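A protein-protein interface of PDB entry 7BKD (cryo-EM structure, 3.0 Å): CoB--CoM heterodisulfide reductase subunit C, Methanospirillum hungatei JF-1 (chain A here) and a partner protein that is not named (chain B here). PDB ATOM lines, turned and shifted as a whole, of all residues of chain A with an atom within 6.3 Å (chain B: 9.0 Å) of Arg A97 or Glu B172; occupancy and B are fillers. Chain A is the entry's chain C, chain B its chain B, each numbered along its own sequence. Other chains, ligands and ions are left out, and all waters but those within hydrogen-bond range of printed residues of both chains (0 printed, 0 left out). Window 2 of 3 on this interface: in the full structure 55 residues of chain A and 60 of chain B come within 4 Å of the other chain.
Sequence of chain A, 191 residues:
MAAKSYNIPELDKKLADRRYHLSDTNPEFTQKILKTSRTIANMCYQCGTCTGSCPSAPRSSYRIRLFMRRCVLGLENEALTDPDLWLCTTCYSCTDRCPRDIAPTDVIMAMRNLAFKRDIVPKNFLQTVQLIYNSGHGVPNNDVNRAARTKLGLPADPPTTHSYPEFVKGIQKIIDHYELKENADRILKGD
Of the 22 printed residues of chain B, 6 touch a printed residue of chain A.
Printed residues of chain B that touch a printed residue of chain A: Lys B161, Pro B162, Lys B163, Lys B164, Thr B171 and Glu B172.
Among the printed residues, 9 pairs touch across the chains.
Among the printed residues, Asp or Glu carboxylates within 4 Å of a Lys or Arg side-chain nitrogen of the other chain: Arg A97 with Glu B172 (3.6 Å).
Of the printed residues of chain B, Ser A93 touches Lys B161.
Of the printed residues of chain B, Thr A95 touches Pro B162 and Lys B164.
Of the printed residues of chain A, Lys B163 touches Asp A96.
Pro B174 touches none of the printed residues of chain A.
The nearest residue of chain B that does not touch Arg A97 is Thr B171 (5.9 Å).
Tyr A92 touches Pro B162.
CG of Pro B162 touches CG2 of Thr A95 (3.9 Å).
Thr A95 touches Lys B164 (CG2 to CE, 3.8 Å).
Pro B162 touches Asp A96.
OG of Ser A93 sits at hydrogen-bond distance from NZ of Lys B161, 2.9 Å away.
The backbone NH (N) of Lys B163 lies within hydrogen-bond range of the side-chain carboxylate (OD1) of Asp A96 (3.0 Å).
The side-chain hydroxyl (OG1) of Thr B171 sits at hydrogen-bond distance from the side-chain carboxylate (OD2) of Asp A96, 3.2 Å away.
The guanidinium group (NE) of Arg A97 lies within salt-bridge range of the side-chain carboxylate (OE2) of Glu B172 (3.6 Å).
The side-chain carboxylate (OD2) of Asp A96 lies close to the side-chain carboxylate (OE2) of Glu B172 (3.4 Å).
The guanidinium group (NH1) of Arg A97 lies within hydrogen-bond range of the side-chain hydroxyl (OG) of Ser A53 (2.8 Å).
The side-chain amino group of Lys B163 lies within salt-bridge range of the side-chain carboxylate of Glu B172, at 3.6 Å.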
ATOM      1  N   THR A  49      24.249 -18.630  -0.529  1.00  0.00           N
ATOM      2  CA  THR A  49      23.431 -18.400  -1.717  1.00  0.00           C
ATOM      3  C   THR A  49      21.995 -18.062  -1.337  1.00  0.00           C
ATOM      4  O   THR A  49      21.365 -17.190  -1.949  1.00  0.00           O
ATOM      5  CB  THR A  49      23.473 -19.631  -2.623  1.00  0.00           C
ATOM      6  OG1 THR A  49      24.817 -19.859  -3.054  1.00  0.00           O
ATOM      7  CG2 THR A  49      22.580 -19.449  -3.839  1.00  0.00           C
ATOM      8  N   CYS A  50      21.476 -18.737  -0.315  1.00  0.00           N
ATOM      9  CA  CYS A  50      20.117 -18.499   0.154  1.00  0.00           C
ATOM     10  C   CYS A  50      19.906 -17.050   0.583  1.00  0.00           C
ATOM     11  O   CYS A  50      18.941 -16.404   0.162  1.00  0.00           O
ATOM     12  CB  CYS A  50      19.806 -19.492   1.274  1.00  0.00           C
ATOM     13  SG  CYS A  50      20.805 -19.343   2.760  1.00  0.00           S
ATOM     14  N   GLY A  52      21.789 -14.496  -0.262  1.00  0.00           N
ATOM     15  CA  GLY A  52      21.980 -13.678  -1.444  1.00  0.00           C
ATOM     16  C   GLY A  52      20.793 -13.675  -2.379  1.00  0.00           C
ATOM     17  O   GLY A  52      20.690 -12.794  -3.236  1.00  0.00           O
ATOM     18  N   SER A  53      19.901 -14.652  -2.247  1.00  0.00           N
ATOM     19  CA  SER A  53      18.694 -14.706  -3.058  1.00  0.00           C
ATOM     20  C   SER A  53      17.510 -13.970  -2.440  1.00  0.00           C
ATOM     21  O   SER A  53      16.551 -13.668  -3.156  1.00  0.00           O
ATOM     22  CB  SER A  53      18.294 -16.164  -3.300  1.00  0.00           C
ATOM     23  OG  SER A  53      19.255 -16.838  -4.086  1.00  0.00           O
ATOM     24  N   CYS A  54      17.558 -13.672  -1.147  1.00  0.00           N
ATOM     25  CA  CYS A  54      16.362 -13.298  -0.397  1.00  0.00           C
ATOM     26  C   CYS A  54      15.926 -11.873  -0.719  1.00  0.00           C
ATOM     27  O   CYS A  54      16.751 -10.958  -0.691  1.00  0.00           O
ATOM     28  CB  CYS A  54      16.605 -13.434   1.098  1.00  0.00           C
ATOM     29  SG  CYS A  54      15.114 -13.327   2.097  1.00  0.00           S
ATOM     30  N   TYR A  92      10.502 -18.948  -2.166  1.00  0.00           N
ATOM     31  CA  TYR A  92      11.185 -20.173  -2.588  1.00  0.00           C
ATOM     32  C   TYR A  92      12.368 -19.902  -3.516  1.00  0.00           C
ATOM     33  O   TYR A  92      12.738 -20.758  -4.319  1.00  0.00           O
ATOM     34  CB  TYR A  92      10.208 -21.155  -3.248  1.00  0.00           C
ATOM     35  CG  TYR A  92       9.435 -21.986  -2.264  1.00  0.00           C
ATOM     36  CD1 TYR A  92       9.893 -23.231  -1.872  1.00  0.00           C
ATOM     37  CD2 TYR A  92       8.252 -21.521  -1.711  1.00  0.00           C
ATOM     38  CE1 TYR A  92       9.191 -23.996  -0.971  1.00  0.00           C
ATOM     39  CE2 TYR A  92       7.547 -22.275  -0.803  1.00  0.00           C
ATOM     40  CZ  TYR A  92       8.022 -23.509  -0.434  1.00  0.00           C
ATOM     41  OH  TYR A  92       7.322 -24.269   0.471  1.00  0.00           O
ATOM     42  N   SER A  93      12.986 -18.726  -3.421  1.00  0.00           N
ATOM     43  CA  SER A  93      14.188 -18.480  -4.215  1.00  0.00           C
ATOM     44  C   SER A  93      15.388 -19.224  -3.640  1.00  0.00           C
ATOM     45  O   SER A  93      16.182 -19.816  -4.384  1.00  0.00           O
ATOM     46  CB  SER A  93      14.469 -16.982  -4.294  1.00  0.00           C
ATOM     47  OG  SER A  93      13.470 -16.319  -5.035  1.00  0.00           O
ATOM     48  N   CYS A  94      15.521 -19.214  -2.314  1.00  0.00           N
ATOM     49  CA  CYS A  94      16.591 -19.953  -1.660  1.00  0.00           C
ATOM     50  C   CYS A  94      16.497 -21.439  -1.971  1.00  0.00           C
ATOM     51  O   CYS A  94      17.495 -22.078  -2.319  1.00  0.00           O
ATOM     52  CB  CYS A  94      16.534 -19.714  -0.154  1.00  0.00           C
ATOM     53  SG  CYS A  94      14.908 -19.986   0.593  1.00  0.00           S
ATOM     54  N   THR A  95      15.297 -22.007  -1.846  1.00  0.00           N
ATOM     55  CA  THR A  95      15.104 -23.412  -2.182  1.00  0.00           C
ATOM     56  C   THR A  95      15.425 -23.661  -3.646  1.00  0.00           C
ATOM     57  O   THR A  95      15.967 -24.712  -4.004  1.00  0.00           O
ATOM     58  CB  THR A  95      13.670 -23.828  -1.866  1.00  0.00           C
ATOM     59  OG1 THR A  95      13.428 -23.667  -0.464  1.00  0.00           O
ATOM     60  CG2 THR A  95      13.429 -25.279  -2.257  1.00  0.00           C
ATOM     61  N   ASP A  96      15.129 -22.687  -4.498  1.00  0.00           N
ATOM     62  CA  ASP A  96      15.374 -22.847  -5.919  1.00  0.00           C
ATOM     63  C   ASP A  96      16.863 -22.836  -6.242  1.00  0.00           C
ATOM     64  O   ASP A  96      17.277 -23.412  -7.253  1.00  0.00           O
ATOM     65  CB  ASP A  96      14.647 -21.746  -6.688  1.00  0.00           C
ATOM     66  CG  ASP A  96      14.730 -21.924  -8.183  1.00  0.00           C
ATOM     67  OD1 ASP A  96      14.036 -22.815  -8.709  1.00  0.00           O
ATOM     68  OD2 ASP A  96      15.486 -21.173  -8.832  1.00  0.00           O
ATOM     69  N   ARG A  97      17.685 -22.198  -5.407  1.00  0.00           N
ATOM     70  CA  ARG A  97      19.095 -22.022  -5.737  1.00  0.00           C
ATOM     71  C   ARG A  97      20.067 -22.783  -4.841  1.00  0.00           C
ATOM     72  O   ARG A  97      21.265 -22.787  -5.132  1.00  0.00           O
ATOM     73  CB  ARG A  97      19.451 -20.534  -5.717  1.00  0.00           C
ATOM     74  CG  ARG A  97      18.621 -19.700  -6.655  1.00  0.00           C
ATOM     75  CD  ARG A  97      19.373 -18.486  -7.121  1.00  0.00           C
ATOM     76  NE  ARG A  97      18.592 -17.688  -8.055  1.00  0.00           N
ATOM     77  CZ  ARG A  97      18.094 -16.491  -7.775  1.00  0.00           C
ATOM     78  NH1 ARG A  97      18.301 -15.951  -6.586  1.00  0.00           N
ATOM     79  NH2 ARG A  97      17.396 -15.833  -8.685  1.00  0.00           N
ATOM     80  N   CYS A  98      19.603 -23.431  -3.783  1.00  0.00           N
ATOM     81  CA  CYS A  98      20.530 -24.038  -2.829  1.00  0.00           C
ATOM     82  C   CYS A  98      21.312 -25.173  -3.483  1.00  0.00           C
ATOM     83  O   CYS A  98      20.714 -26.050  -4.113  1.00  0.00           O
ATOM     84  CB  CYS A  98      19.786 -24.555  -1.603  1.00  0.00           C
ATOM     85  SG  CYS A  98      20.827 -25.441  -0.426  1.00  0.00           S
ATOM     86  N   PRO A  99      22.641 -25.196  -3.351  1.00  0.00           N
ATOM     87  CA  PRO A  99      23.433 -26.253  -3.998  1.00  0.00           C
ATOM     88  C   PRO A  99      23.373 -27.587  -3.282  1.00  0.00           C
ATOM     89  O   PRO A  99      23.863 -28.581  -3.827  1.00  0.00           O
ATOM     90  CB  PRO A  99      24.862 -25.688  -3.974  1.00  0.00           C
ATOM     91  CG  PRO A  99      24.749 -24.300  -3.378  1.00  0.00           C
ATOM     92  CD  PRO A  99      23.492 -24.263  -2.601  1.00  0.00           C
ATOM     93  N   ARG A 100      22.804 -27.641  -2.082  1.00  0.00           N
ATOM     94  CA  ARG A 100      22.723 -28.860  -1.296  1.00  0.00           C
ATOM     95  C   ARG A 100      21.344 -29.506  -1.343  1.00  0.00           C
ATOM     96  O   ARG A 100      21.098 -30.453  -0.592  1.00  0.00           O
ATOM     97  CB  ARG A 100      23.111 -28.565   0.152  1.00  0.00           C
ATOM     98  CG  ARG A 100      24.590 -28.700   0.436  1.00  0.00           C
ATOM     99  CD  ARG A 100      24.988 -30.148   0.601  1.00  0.00           C
ATOM    100  NE  ARG A 100      26.430 -30.339   0.495  1.00  0.00           N
ATOM    101  CZ  ARG A 100      27.251 -30.452   1.531  1.00  0.00           C
ATOM    102  NH1 ARG A 100      26.782 -30.378   2.768  1.00  0.00           N
ATOM    103  NH2 ARG A 100      28.547 -30.623   1.331  1.00  0.00           N
ATOM    104  N   TYR B 155       5.143 -12.745 -12.892  1.00  0.00           N
ATOM    105  CA  TYR B 155       4.890 -14.179 -12.841  1.00  0.00           C
ATOM    106  C   TYR B 155       4.445 -14.643 -11.465  1.00  0.00           C
ATOM    107  O   TYR B 155       3.717 -15.635 -11.359  1.00  0.00           O
ATOM    108  CB  TYR B 155       6.144 -14.947 -13.256  1.00  0.00           C
ATOM    109  CG  TYR B 155       6.368 -15.014 -14.745  1.00  0.00           C
ATOM    110  CD1 TYR B 155       6.184 -16.199 -15.440  1.00  0.00           C
ATOM    111  CD2 TYR B 155       6.772 -13.894 -15.456  1.00  0.00           C
ATOM    112  CE1 TYR B 155       6.392 -16.268 -16.800  1.00  0.00           C
ATOM    113  CE2 TYR B 155       6.983 -13.953 -16.814  1.00  0.00           C
ATOM    114  CZ  TYR B 155       6.791 -15.142 -17.484  1.00  0.00           C
ATOM    115  OH  TYR B 155       6.997 -15.200 -18.840  1.00  0.00           O
ATOM    116  N   GLY B 156       4.865 -13.956 -10.410  1.00  0.00           N
ATOM    117  CA  GLY B 156       4.656 -14.451  -9.069  1.00  0.00           C
ATOM    118  C   GLY B 156       5.679 -15.510  -8.720  1.00  0.00           C
ATOM    119  O   GLY B 156       6.621 -15.784  -9.460  1.00  0.00           O
ATOM    120  N   MET B 160       5.785 -21.136 -10.372  1.00  0.00           N
ATOM    121  CA  MET B 160       6.934 -21.771 -10.996  1.00  0.00           C
ATOM    122  C   MET B 160       8.041 -22.178 -10.034  1.00  0.00           C
ATOM    123  O   MET B 160       8.860 -23.022 -10.397  1.00  0.00           O
ATOM    124  CB  MET B 160       7.530 -20.853 -12.071  1.00  0.00           C
ATOM    125  CG  MET B 160       6.613 -20.642 -13.259  1.00  0.00           C
ATOM    126  SD  MET B 160       7.295 -19.504 -14.467  1.00  0.00           S
ATOM    127  CE  MET B 160       8.621 -20.499 -15.136  1.00  0.00           C
ATOM    128  N   LYS B 161       8.084 -21.628  -8.837  1.00  0.00           N
ATOM    129  CA  LYS B 161       9.195 -22.001  -7.982  1.00  0.00           C
ATOM    130  C   LYS B 161       8.737 -22.941  -6.873  1.00  0.00           C
ATOM    131  O   LYS B 161       7.604 -22.839  -6.397  1.00  0.00           O
ATOM    132  CB  LYS B 161       9.848 -20.763  -7.361  1.00  0.00           C
ATOM    133  CG  LYS B 161      10.627 -19.925  -8.353  1.00  0.00           C
ATOM    134  CD  LYS B 161      11.335 -18.778  -7.660  1.00  0.00           C
ATOM    135  CE  LYS B 161      10.404 -17.604  -7.445  1.00  0.00           C
ATOM    136  NZ  LYS B 161      10.941 -16.672  -6.427  1.00  0.00           N
ATOM    137  N   PRO B 162       9.590 -23.881  -6.439  1.00  0.00           N
ATOM    138  CA  PRO B 162      10.935 -24.158  -6.959  1.00  0.00           C
ATOM    139  C   PRO B 162      10.932 -25.064  -8.194  1.00  0.00           C
ATOM    140  O   PRO B 162       9.939 -25.738  -8.449  1.00  0.00           O
ATOM    141  CB  PRO B 162      11.631 -24.849  -5.783  1.00  0.00           C
ATOM    142  CG  PRO B 162      10.535 -25.329  -4.875  1.00  0.00           C
ATOM    143  CD  PRO B 162       9.224 -24.780  -5.332  1.00  0.00           C
ATOM    144  N   LYS B 163      12.041 -25.078  -8.941  1.00  0.00           N
ATOM    145  CA  LYS B 163      12.148 -25.956 -10.103  1.00  0.00           C
ATOM    146  C   LYS B 163      11.957 -27.417  -9.719  1.00  0.00           C
ATOM    147  O   LYS B 163      11.270 -28.168 -10.419  1.00  0.00           O
ATOM    148  CB  LYS B 163      13.506 -25.790 -10.783  1.00  0.00           C
ATOM    149  CG  LYS B 163      13.789 -24.455 -11.421  1.00  0.00           C
ATOM    150  CD  LYS B 163      15.157 -24.500 -12.088  1.00  0.00           C
ATOM    151  CE  LYS B 163      16.068 -23.398 -11.601  1.00  0.00           C
ATOM    152  NZ  LYS B 163      16.554 -22.565 -12.737  1.00  0.00           N
ATOM    153  N   LYS B 164      12.572 -27.840  -8.617  1.00  0.00           N
ATOM    154  CA  LYS B 164      12.537 -29.233  -8.196  1.00  0.00           C
ATOM    155  C   LYS B 164      11.153 -29.692  -7.756  1.00  0.00           C
ATOM    156  O   LYS B 164      10.951 -30.898  -7.581  1.00  0.00           O
ATOM    157  CB  LYS B 164      13.553 -29.443  -7.074  1.00  0.00           C
ATOM    158  CG  LYS B 164      13.093 -28.967  -5.707  1.00  0.00           C
ATOM    159  CD  LYS B 164      14.280 -28.821  -4.767  1.00  0.00           C
ATOM    160  CE  LYS B 164      13.862 -28.932  -3.309  1.00  0.00           C
ATOM    161  NZ  LYS B 164      15.046 -28.951  -2.404  1.00  0.00           N
ATOM    162  N   PHE B 168       7.457 -26.142 -14.886  1.00  0.00           N
ATOM    163  CA  PHE B 168       7.294 -25.070 -15.857  1.00  0.00           C
ATOM    164  C   PHE B 168       8.602 -24.610 -16.481  1.00  0.00           C
ATOM    165  O   PHE B 168       8.595 -23.648 -17.251  1.00  0.00           O
ATOM    166  CB  PHE B 168       6.582 -23.885 -15.204  1.00  0.00           C
ATOM    167  CG  PHE B 168       5.257 -24.243 -14.615  1.00  0.00           C
ATOM    168  CD1 PHE B 168       4.129 -24.275 -15.407  1.00  0.00           C
ATOM    169  CD2 PHE B 168       5.143 -24.579 -13.278  1.00  0.00           C
ATOM    170  CE1 PHE B 168       2.913 -24.612 -14.875  1.00  0.00           C
ATOM    171  CE2 PHE B 168       3.921 -24.924 -12.742  1.00  0.00           C
ATOM    172  CZ  PHE B 168       2.807 -24.940 -13.540  1.00  0.00           C
ATOM    173  N   GLY B 169       9.717 -25.262 -16.171  1.00  0.00           N
ATOM    174  CA  GLY B 169      10.976 -24.901 -16.788  1.00  0.00           C
ATOM    175  C   GLY B 169      11.788 -23.901 -15.993  1.00  0.00           C
ATOM    176  O   GLY B 169      11.769 -23.919 -14.760  1.00  0.00           O
ATOM    177  N   ASP B 170      12.503 -23.021 -16.690  1.00  0.00           N
ATOM    178  CA  ASP B 170      13.406 -22.093 -16.024  1.00  0.00           C
ATOM    179  C   ASP B 170      12.620 -21.024 -15.279  1.00  0.00           C
ATOM    180  O   ASP B 170      11.759 -20.356 -15.856  1.00  0.00           O
ATOM    181  CB  ASP B 170      14.343 -21.440 -17.039  1.00  0.00           C
ATOM    182  CG  ASP B 170      13.605 -20.867 -18.236  1.00  0.00           C
ATOM    183  OD1 ASP B 170      12.639 -21.506 -18.702  1.00  0.00           O
ATOM    184  OD2 ASP B 170      13.994 -19.782 -18.717  1.00  0.00           O
ATOM    185  N   THR B 171      12.941 -20.846 -14.000  1.00  0.00           N
ATOM    186  CA  THR B 171      12.283 -19.872 -13.145  1.00  0.00           C
ATOM    187  C   THR B 171      13.061 -18.569 -13.048  1.00  0.00           C
ATOM    188  O   THR B 171      12.934 -17.851 -12.051  1.00  0.00           O
ATOM    189  CB  THR B 171      12.083 -20.454 -11.747  1.00  0.00           C
ATOM    190  OG1 THR B 171      13.356 -20.594 -11.105  1.00  0.00           O
ATOM    191  CG2 THR B 171      11.426 -21.811 -11.834  1.00  0.00           C
ATOM    192  N   GLU B 172      13.863 -18.247 -14.058  1.00  0.00           N
ATOM    193  CA  GLU B 172      14.843 -17.182 -13.912  1.00  0.00           C
ATOM    194  C   GLU B 172      14.821 -16.225 -15.098  1.00  0.00           C
ATOM    195  O   GLU B 172      15.188 -15.053 -14.965  1.00  0.00           O
ATOM    196  CB  GLU B 172      16.213 -17.819 -13.697  1.00  0.00           C
ATOM    197  CG  GLU B 172      16.257 -18.539 -12.350  1.00  0.00           C
ATOM    198  CD  GLU B 172      17.560 -19.224 -12.071  1.00  0.00           C
ATOM    199  OE1 GLU B 172      18.404 -19.257 -12.980  1.00  0.00           O
ATOM    200  OE2 GLU B 172      17.736 -19.730 -10.943  1.00  0.00           O
ATOM    201  N   ASN B 173      14.373 -16.705 -16.253  1.00  0.00           N
ATOM    202  CA  ASN B 173      13.960 -15.833 -17.354  1.00  0.00           C
ATOM    203  C   ASN B 173      12.887 -16.525 -18.184  1.00  0.00           C
ATOM    204  O   ASN B 173      13.073 -16.788 -19.375  1.00  0.00           O
ATOM    205  CB  ASN B 173      15.150 -15.430 -18.221  1.00  0.00           C
ATOM    206  CG  ASN B 173      14.837 -14.243 -19.111  1.00  0.00           C
ATOM    207  OD1 ASN B 173      14.171 -13.300 -18.690  1.00  0.00           O
ATOM    208  ND2 ASN B 173      15.307 -14.289 -20.350  1.00  0.00           N
ATOM    209  N   PRO B 174      11.739 -16.832 -17.582  1.00  0.00           N
ATOM    210  CA  PRO B 174      10.647 -17.413 -18.363  1.00  0.00           C
ATOM    211  C   PRO B 174      10.104 -16.415 -19.367  1.00  0.00           C
ATOM    212  O   PRO B 174      10.164 -15.200 -19.171  1.00  0.00           O
ATOM    213  CB  PRO B 174       9.598 -17.763 -17.303  1.00  0.00           C
ATOM    214  CG  PRO B 174       9.862 -16.815 -16.206  1.00  0.00           C
ATOM    215  CD  PRO B 174      11.343 -16.612 -16.180  1.00  0.00           C
ATOM    216  N   MET B 175       9.573 -16.947 -20.462  1.00  0.00           N
ATOM    217  CA  MET B 175       9.005 -16.122 -21.512  1.00  0.00           C
ATOM    218  C   MET B 175       7.606 -16.561 -21.913  1.00  0.00           C
ATOM    219  O   MET B 175       7.036 -15.973 -22.836  1.00  0.00           O
ATOM    220  CB  MET B 175       9.908 -16.129 -22.755  1.00  0.00           C
ATOM    221  CG  MET B 175      11.361 -15.765 -22.496  1.00  0.00           C
ATOM    222  SD  MET B 175      11.583 -14.124 -21.782  1.00  0.00           S
ATOM    223  CE  MET B 175      10.679 -13.117 -22.952  1.00  0.00           C
ATOM    224  N   TRP B 176       7.044 -17.576 -21.258  1.00  0.00           N
ATOM    225  CA  TRP B 176       5.803 -18.164 -21.745  1.00  0.00           C
ATOM    226  C   TRP B 176       4.616 -17.245 -21.484  1.00  0.00           C
ATOM    227  O   TRP B 176       3.779 -17.020 -22.369  1.00  0.00           O
ATOM    228  CB  TRP B 176       5.591 -19.531 -21.096  1.00  0.00           C
ATOM    229  CG  TRP B 176       5.478 -19.550 -19.608  1.00  0.00           C
ATOM    230  CD1 TRP B 176       6.489 -19.657 -18.704  1.00  0.00           C
ATOM    231  CD2 TRP B 176       4.264 -19.528 -18.852  1.00  0.00           C
ATOM    232  NE1 TRP B 176       5.981 -19.669 -17.428  1.00  0.00           N
ATOM    233  CE2 TRP B 176       4.615 -19.594 -17.494  1.00  0.00           C
ATOM    234  CE3 TRP B 176       2.911 -19.449 -19.196  1.00  0.00           C
ATOM    235  CZ2 TRP B 176       3.667 -19.579 -16.478  1.00  0.00           C
ATOM    236  CZ3 TRP B 176       1.971 -19.436 -18.188  1.00  0.00           C
ATOM    237  CH2 TRP B 176       2.352 -19.500 -16.845  1.00  0.00           C
ATOM    238  N   GLN B 190      10.284  -5.761 -20.940  1.00  0.00           N
ATOM    239  CA  GLN B 190      11.207  -6.358 -19.989  1.00  0.00           C
ATOM    240  C   GLN B 190      11.683  -5.290 -19.014  1.00  0.00           C
ATOM    241  O   GLN B 190      12.003  -4.167 -19.415  1.00  0.00           O
ATOM    242  CB  GLN B 190      12.401  -6.988 -20.709  1.00  0.00           C
ATOM    243  CG  GLN B 190      12.099  -8.315 -21.387  1.00  0.00           C
ATOM    244  CD  GLN B 190      11.662  -9.386 -20.416  1.00  0.00           C
ATOM    245  OE1 GLN B 190      12.376  -9.706 -19.469  1.00  0.00           O
ATOM    246  NE2 GLN B 190      10.478  -9.942 -20.639  1.00  0.00           N
ATOM    247  N   TYR B 191      11.713  -5.643 -17.734  1.00  0.00           N
ATOM    248  CA  TYR B 191      12.174  -4.749 -16.683  1.00  0.00           C
ATOM    249  C   TYR B 191      13.104  -5.522 -15.761  1.00  0.00           C
ATOM    250  O   TYR B 191      13.024  -6.748 -15.667  1.00  0.00           O
ATOM    251  CB  TYR B 191      10.995  -4.145 -15.896  1.00  0.00           C
ATOM    252  CG  TYR B 191      10.077  -5.154 -15.246  1.00  0.00           C
ATOM    253  CD1 TYR B 191       9.145  -5.862 -15.993  1.00  0.00           C
ATOM    254  CD2 TYR B 191      10.126  -5.381 -13.881  1.00  0.00           C
ATOM    255  CE1 TYR B 191       8.307  -6.778 -15.402  1.00  0.00           C
ATOM    256  CE2 TYR B 191       9.286  -6.291 -13.281  1.00  0.00           C
ATOM    257  CZ  TYR B 191       8.379  -6.988 -14.046  1.00  0.00           C
ATOM    258  OH  TYR B 191       7.544  -7.899 -13.450  1.00  0.00           O
ATOM    259  N   ASN B 193      15.047  -7.375 -12.858  1.00  0.00           N
ATOM    260  CA  ASN B 193      14.632  -8.240 -11.758  1.00  0.00           C
ATOM    261  C   ASN B 193      13.134  -8.531 -11.822  1.00  0.00           C
ATOM    262  O   ASN B 193      12.408  -8.418 -10.833  1.00  0.00           O
ATOM    263  CB  ASN B 193      15.026  -7.632 -10.411  1.00  0.00           C
ATOM    264  CG  ASN B 193      15.136  -8.670  -9.318  1.00  0.00           C
ATOM    265  OD1 ASN B 193      15.371  -9.846  -9.587  1.00  0.00           O
ATOM    266  ND2 ASN B 193      14.967  -8.241  -8.074  1.00  0.00           N
ATOM    267  N   LYS B 194      12.671  -8.923 -13.010  1.00  0.00           N
ATOM    268  CA  LYS B 194      11.247  -9.152 -13.223  1.00  0.00           C
ATOM    269  C   LYS B 194      10.728 -10.386 -12.502  1.00  0.00           C
ATOM    270  O   LYS B 194       9.510 -10.561 -12.422  1.00  0.00           O
ATOM    271  CB  LYS B 194      10.942  -9.262 -14.718  1.00  0.00           C
ATOM    272  CG  LYS B 194      11.229 -10.615 -15.341  1.00  0.00           C
ATOM    273  CD  LYS B 194      10.658 -10.682 -16.746  1.00  0.00           C
ATOM    274  CE  LYS B 194      11.065 -11.953 -17.478  1.00  0.00           C
ATOM    275  NZ  LYS B 194      10.457 -13.178 -16.906  1.00  0.00           N
ATOM    276  N   MET B 195      11.604 -11.234 -11.978  1.00  0.00           N
ATOM    277  CA  MET B 195      11.199 -12.422 -11.246  1.00  0.00           C
ATOM    278  C   MET B 195      11.141 -12.191  -9.743  1.00  0.00           C
ATOM    279  O   MET B 195      11.041 -13.156  -8.980  1.00  0.00           O
ATOM    280  CB  MET B 195      12.147 -13.580 -11.558  1.00  0.00           C
ATOM    281  CG  MET B 195      12.070 -14.066 -12.993  1.00  0.00           C
ATOM    282  SD  MET B 195      10.375 -14.197 -13.592  1.00  0.00           S
ATOM    283  CE  MET B 195       9.833 -15.661 -12.720  1.00  0.00           C
ATOM    284  N   GLN B 196      11.205 -10.938  -9.306  1.00  0.00           N
ATOM    285  CA  GLN B 196      11.219 -10.616  -7.889  1.00  0.00           C
ATOM    286  C   GLN B 196       9.838 -10.803  -7.272  1.00  0.00           C
ATOM    287  O   GLN B 196       8.816 -10.523  -7.902  1.00  0.00           O
ATOM    288  CB  GLN B 196      11.696  -9.178  -7.693  1.00  0.00           C
ATOM    289  CG  GLN B 196      11.794  -8.725  -6.254  1.00  0.00           C
ATOM    290  CD  GLN B 196      11.766  -7.222  -6.125  1.00  0.00           C
ATOM    291  OE1 GLN B 196      11.183  -6.681  -5.191  1.00  0.00           O
ATOM    292  NE2 GLN B 196      12.386  -6.536  -7.075  1.00  0.00           N
